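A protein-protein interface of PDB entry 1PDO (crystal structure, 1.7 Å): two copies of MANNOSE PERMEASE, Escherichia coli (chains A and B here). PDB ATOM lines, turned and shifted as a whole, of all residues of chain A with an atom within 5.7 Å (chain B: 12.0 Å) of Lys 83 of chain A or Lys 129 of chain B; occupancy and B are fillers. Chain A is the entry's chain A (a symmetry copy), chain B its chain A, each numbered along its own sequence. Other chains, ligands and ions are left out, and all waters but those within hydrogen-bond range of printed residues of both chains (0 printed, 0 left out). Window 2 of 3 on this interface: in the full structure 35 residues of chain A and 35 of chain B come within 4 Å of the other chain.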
ATOM      1  N   ARG A  78      16.744  13.231 -17.902  1.00  0.00           N
ATOM      2  CA  ARG A  78      15.860  13.097 -19.054  1.00  0.00           C
ATOM      3  C   ARG A  78      16.479  13.633 -20.349  1.00  0.00           C
ATOM      4  O   ARG A  78      16.204  13.119 -21.420  1.00  0.00           O
ATOM      5  CB  ARG A  78      14.522  13.731 -18.750  1.00  0.00           C
ATOM      6  CG  ARG A  78      13.733  12.899 -17.762  1.00  0.00           C
ATOM      7  CD  ARG A  78      12.255  13.135 -17.946  1.00  0.00           C
ATOM      8  NE  ARG A  78      11.592  13.720 -16.781  1.00  0.00           N
ATOM      9  CZ  ARG A  78      10.510  14.495 -16.861  1.00  0.00           C
ATOM     10  NH1 ARG A  78       9.983  14.781 -18.058  1.00  0.00           N
ATOM     11  NH2 ARG A  78       9.939  14.954 -15.748  1.00  0.00           N
ATOM     12  N   ILE A  79      17.356  14.627 -20.238  1.00  0.00           N
ATOM     13  CA  ILE A  79      18.032  15.201 -21.394  1.00  0.00           C
ATOM     14  C   ILE A  79      19.178  14.321 -21.907  1.00  0.00           C
ATOM     15  O   ILE A  79      19.319  14.115 -23.108  1.00  0.00           O
ATOM     16  CB  ILE A  79      18.598  16.603 -21.031  1.00  0.00           C
ATOM     17  CG1 ILE A  79      17.425  17.562 -20.728  1.00  0.00           C
ATOM     18  CG2 ILE A  79      19.602  17.106 -22.096  1.00  0.00           C
ATOM     19  CD1 ILE A  79      17.852  18.974 -20.286  1.00  0.00           C
ATOM     20  N   VAL A  80      19.974  13.757 -21.002  1.00  0.00           N
ATOM     21  CA  VAL A  80      21.122  12.988 -21.450  1.00  0.00           C
ATOM     22  C   VAL A  80      20.825  11.586 -21.898  1.00  0.00           C
ATOM     23  O   VAL A  80      21.667  11.031 -22.601  1.00  0.00           O
ATOM     24  CB  VAL A  80      22.243  12.910 -20.412  1.00  0.00           C
ATOM     25  CG1 VAL A  80      22.446  14.263 -19.771  1.00  0.00           C
ATOM     26  CG2 VAL A  80      21.955  11.834 -19.377  1.00  0.00           C
ATOM     27  N   VAL A  81      19.645  11.047 -21.538  1.00  0.00           N
ATOM     28  CA  VAL A  81      19.233   9.653 -21.847  1.00  0.00           C
ATOM     29  C   VAL A  81      19.736   8.911 -23.091  1.00  0.00           C
ATOM     30  O   VAL A  81      20.226   7.780 -22.966  1.00  0.00           O
ATOM     31  CB  VAL A  81      17.713   9.417 -21.743  1.00  0.00           C
ATOM     32  CG1 VAL A  81      17.268   9.476 -20.298  1.00  0.00           C
ATOM     33  CG2 VAL A  81      16.971  10.398 -22.622  1.00  0.00           C
ATOM     34  N   ASP A  82      19.547   9.447 -24.289  1.00  0.00           N
ATOM     35  CA  ASP A  82      20.087   8.696 -25.432  1.00  0.00           C
ATOM     36  C   ASP A  82      20.989   9.588 -26.237  1.00  0.00           C
ATOM     37  O   ASP A  82      21.008   9.560 -27.466  1.00  0.00           O
ATOM     38  CB  ASP A  82      19.001   8.088 -26.314  1.00  0.00           C
ATOM     39  CG  ASP A  82      17.605   8.429 -25.846  1.00  0.00           C
ATOM     40  OD1 ASP A  82      17.332   9.634 -25.597  1.00  0.00           O
ATOM     41  OD2 ASP A  82      16.785   7.484 -25.736  1.00  0.00           O
ATOM     42  N   LYS A  83      21.746  10.390 -25.518  1.00  0.00           N
ATOM     43  CA  LYS A  83      22.645  11.303 -26.154  1.00  0.00           C
ATOM     44  C   LYS A  83      24.065  10.897 -25.874  1.00  0.00           C
ATOM     45  O   LYS A  83      24.415  10.615 -24.730  1.00  0.00           O
ATOM     46  CB  LYS A  83      22.407  12.704 -25.627  1.00  0.00           C
ATOM     47  CG  LYS A  83      21.633  13.563 -26.544  1.00  0.00           C
ATOM     48  CD  LYS A  83      20.274  13.786 -26.003  1.00  0.00           C
ATOM     49  CE  LYS A  83      19.890  15.248 -26.130  1.00  0.00           C
ATOM     50  NZ  LYS A  83      18.496  15.475 -25.623  1.00  0.00           N
ATOM     51  N   GLU A  84      24.876  10.888 -26.926  1.00  0.00           N
ATOM     52  CA  GLU A  84      26.286  10.542 -26.839  1.00  0.00           C
ATOM     53  C   GLU A  84      26.997  11.758 -26.295  1.00  0.00           C
ATOM     54  O   GLU A  84      26.673  12.895 -26.642  1.00  0.00           O
ATOM     55  CB  GLU A  84      26.868  10.184 -28.219  1.00  0.00           C
ATOM     56  N   HIS A  85      27.975  11.505 -25.442  1.00  0.00           N
ATOM     57  CA  HIS A  85      28.730  12.571 -24.851  1.00  0.00           C
ATOM     58  C   HIS A  85      27.929  13.533 -23.970  1.00  0.00           C
ATOM     59  O   HIS A  85      28.219  14.717 -23.927  1.00  0.00           O
ATOM     60  CB  HIS A  85      29.476  13.305 -25.914  1.00  0.00           C
ATOM     61  CG  HIS A  85      30.491  12.448 -26.600  1.00  0.00           C
ATOM     62  ND1 HIS A  85      31.190  12.853 -27.716  1.00  0.00           N
ATOM     63  CD2 HIS A  85      30.937  11.205 -26.302  1.00  0.00           C
ATOM     64  CE1 HIS A  85      32.033  11.896 -28.070  1.00  0.00           C
ATOM     65  NE2 HIS A  85      31.897  10.885 -27.231  1.00  0.00           N
ATOM     66  N   TYR A  86      26.926  12.995 -23.290  1.00  0.00           N
ATOM     67  CA  TYR A  86      26.114  13.743 -22.336  1.00  0.00           C
ATOM     68  C   TYR A  86      26.140  12.924 -21.052  1.00  0.00           C
ATOM     69  O   TYR A  86      25.824  11.736 -21.046  1.00  0.00           O
ATOM     70  CB  TYR A  86      24.644  13.871 -22.785  1.00  0.00           C
ATOM     71  CG  TYR A  86      24.341  15.053 -23.697  1.00  0.00           C
ATOM     72  CD1 TYR A  86      25.040  15.238 -24.877  1.00  0.00           C
ATOM     73  CD2 TYR A  86      23.339  15.975 -23.371  1.00  0.00           C
ATOM     74  CE1 TYR A  86      24.746  16.280 -25.708  1.00  0.00           C
ATOM     75  CE2 TYR A  86      23.036  17.026 -24.203  1.00  0.00           C
ATOM     76  CZ  TYR A  86      23.746  17.176 -25.365  1.00  0.00           C
ATOM     77  OH  TYR A  86      23.466  18.220 -26.202  1.00  0.00           O
ATOM     78  N   GLU A  87      26.426  13.581 -19.935  1.00  0.00           N
ATOM     79  CA  GLU A  87      26.484  12.879 -18.667  1.00  0.00           C
ATOM     80  C   GLU A  87      26.009  13.788 -17.533  1.00  0.00           C
ATOM     81  O   GLU A  87      26.000  15.010 -17.667  1.00  0.00           O
ATOM     82  CB  GLU A  87      27.926  12.420 -18.406  1.00  0.00           C
ATOM     83  CG  GLU A  87      28.147  11.707 -17.050  1.00  0.00           C
ATOM     84  CD  GLU A  87      27.330  10.422 -16.911  1.00  0.00           C
ATOM     85  OE1 GLU A  87      26.086  10.450 -16.792  1.00  0.00           O
ATOM     86  OE2 GLU A  87      27.963   9.352 -16.942  1.00  0.00           O
ATOM     87  N   VAL A  88      25.521  13.163 -16.464  1.00  0.00           N
ATOM     88  CA  VAL A  88      25.095  13.899 -15.277  1.00  0.00           C
ATOM     89  C   VAL A  88      25.940  13.348 -14.098  1.00  0.00           C
ATOM     90  O   VAL A  88      26.045  12.129 -13.900  1.00  0.00           O
ATOM     91  CB  VAL A  88      23.616  13.628 -14.876  1.00  0.00           C
ATOM     92  CG1 VAL A  88      23.202  14.620 -13.752  1.00  0.00           C
ATOM     93  CG2 VAL A  88      22.677  13.692 -16.056  1.00  0.00           C
ATOM     94  N   GLY B 124      28.328  10.841  -2.232  1.00  0.00           N
ATOM     95  CA  GLY B 124      27.404  11.702  -2.960  1.00  0.00           C
ATOM     96  C   GLY B 124      27.871  12.039  -4.379  1.00  0.00           C
ATOM     97  O   GLY B 124      27.083  12.532  -5.183  1.00  0.00           O
ATOM     98  N   VAL B 125      29.155  11.826  -4.666  1.00  0.00           N
ATOM     99  CA  VAL B 125      29.702  12.110  -6.002  1.00  0.00           C
ATOM    100  C   VAL B 125      29.514  10.832  -6.821  1.00  0.00           C
ATOM    101  O   VAL B 125      30.166   9.805  -6.583  1.00  0.00           O
ATOM    102  CB  VAL B 125      31.161  12.515  -5.918  1.00  0.00           C
ATOM    103  CG1 VAL B 125      31.735  12.701  -7.312  1.00  0.00           C
ATOM    104  CG2 VAL B 125      31.296  13.788  -5.077  1.00  0.00           C
ATOM    105  N   LYS B 126      28.660  10.909  -7.822  1.00  0.00           N
ATOM    106  CA  LYS B 126      28.305   9.715  -8.561  1.00  0.00           C
ATOM    107  C   LYS B 126      27.819  10.135  -9.950  1.00  0.00           C
ATOM    108  O   LYS B 126      27.048  11.089 -10.057  1.00  0.00           O
ATOM    109  CB  LYS B 126      27.116   9.156  -7.789  1.00  0.00           C
ATOM    110  CG  LYS B 126      26.836   7.716  -7.840  1.00  0.00           C
ATOM    111  CD  LYS B 126      25.544   7.472  -7.046  1.00  0.00           C
ATOM    112  CE  LYS B 126      25.417   8.392  -5.807  1.00  0.00           C
ATOM    113  N   ALA B 127      28.247   9.424 -10.992  1.00  0.00           N
ATOM    114  CA  ALA B 127      27.803   9.683 -12.368  1.00  0.00           C
ATOM    115  C   ALA B 127      26.631   8.777 -12.717  1.00  0.00           C
ATOM    116  O   ALA B 127      26.480   7.671 -12.189  1.00  0.00           O
ATOM    117  CB  ALA B 127      28.944   9.508 -13.356  1.00  0.00           C
ATOM    118  N   LEU B 128      25.731   9.302 -13.541  1.00  0.00           N
ATOM    119  CA  LEU B 128      24.548   8.570 -13.952  1.00  0.00           C
ATOM    120  C   LEU B 128      24.911   7.363 -14.825  1.00  0.00           C
ATOM    121  O   LEU B 128      24.637   6.210 -14.475  1.00  0.00           O
ATOM    122  CB  LEU B 128      23.603   9.512 -14.723  1.00  0.00           C
ATOM    123  CG  LEU B 128      22.378   8.863 -15.380  1.00  0.00           C
ATOM    124  CD1 LEU B 128      21.488   8.226 -14.333  1.00  0.00           C
ATOM    125  CD2 LEU B 128      21.607   9.908 -16.149  1.00  0.00           C
ATOM    126  N   LYS B 129      25.573   7.641 -15.936  1.00  0.00           N
ATOM    127  CA  LYS B 129      25.956   6.607 -16.893  1.00  0.00           C
ATOM    128  C   LYS B 129      27.273   5.850 -16.647  1.00  0.00           C
ATOM    129  O   LYS B 129      28.267   6.388 -16.075  1.00  0.00           O
ATOM    130  CB  LYS B 129      25.979   7.197 -18.307  1.00  0.00           C
ATOM    131  CG  LYS B 129      24.712   7.931 -18.762  1.00  0.00           C
ATOM    132  CD  LYS B 129      25.045   8.688 -20.050  1.00  0.00           C
ATOM    133  CE  LYS B 129      23.839   9.282 -20.700  1.00  0.00           C
ATOM    134  NZ  LYS B 129      24.160   9.654 -22.096  1.00  0.00           N
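The side-chain amino group (NZ) of Lys 129 of chain B lies within hydrogen-bond range of the backbone carbonyl oxygen (O) of Val 80 of chain A (2.9 Å). OE1 of Glu 87 of chain A sits close to N of Leu 128 of chain B (3.5 Å). N of Lys 129 of chain B lies within hydrogen-bond range of OE1 of Glu 87 of chain A, at 3.0 Å. The backbone carbonyl oxygen (O) of Val 88 of chain A is in hydrogen-bond range of the backbone NH (N) of Leu 128 of chain B, at 2.9 Å. The side-chain amino group (NZ) of Lys 129 of chain B sits at hydrogen-bond distance from the backbone carbonyl oxygen (O) of Lys 83 of chain A, 2.8 Å away. The backbone carbonyl oxygen (O) of Tyr 86 of chain A lies within hydrogen-bond range of the side-chain amino group (NZ) of Lys 129 of chain B (2.9 Å).
The side-chain amino group of Lys 83 of chain A is in hydrogen-bond range of the backbone carbonyl oxygen of Ile 79 of chain A.
CD2 of Leu 128 of chain B touches CG2 of Val 80 of chain A, at 3.8 Å. Glu 87 of chain A touches Ala 127 of chain B (OE2 to CB, 3.7 Å). Val 88 of chain A touches Ala 127 of chain B (O to CA, 3.4 Å).
No residue of chain B comes within 4 Å of Ile 79 of chain A. Of chain B, only Leu 128 and Lys 129 come within 4 Å of Val 80 of chain A. No residue of chain B comes within 4 Å of Val 81 of chain A. No residue of chain B comes within 4 Å of Asp 82 of chain A. No residue of chain B comes within 4 Å of Glu 84 of chain A. Of the printed residues of chain B, Tyr 86 of chain A touches Lys 129. Glu 87 of chain A touches just these residues of chain B: Ala 127, Leu 128 and Lys 129. Val 88 of chain A touches just these residues of chain B: Ala 127 (3.4 Å) and Leu 128 (2.9 Å). Printed residues of chain A within 4 Å of Leu 128 of chain B: Val 80, Glu 87 and Val 88. Printed residues of chain A within 4 Å of Ala 127 of chain B: Glu 87 and Val 88. Val 125 of chain B touches none of the printed residues of chain A. The nearest residue of chain B that does not touch Lys 83 of chain A is Leu 128 of chain B (9.1 Å).
Hydrophobic or aromatic side chains of chain B that line the printed part of chain A: Ala 127 and Leu 128. Along chain B the printed residues that touch a printed residue of chain A span positions 127 to 129. Printed residues of chain A that touch a printed residue of chain B: Val 80, Lys 83, Tyr 86, Glu 87 and Val 88. Among the printed residues, 9 pairs touch across the chains. Among the printed residues, no Asp or Glu carboxylate lies within 4 Å of a Lys or Arg side-chain nitrogen of the other chain.
No position is printed for both chains. Of the 9 pairs that touch across the chains among the printed residues, none has its exchanged pair printed and touching as well.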
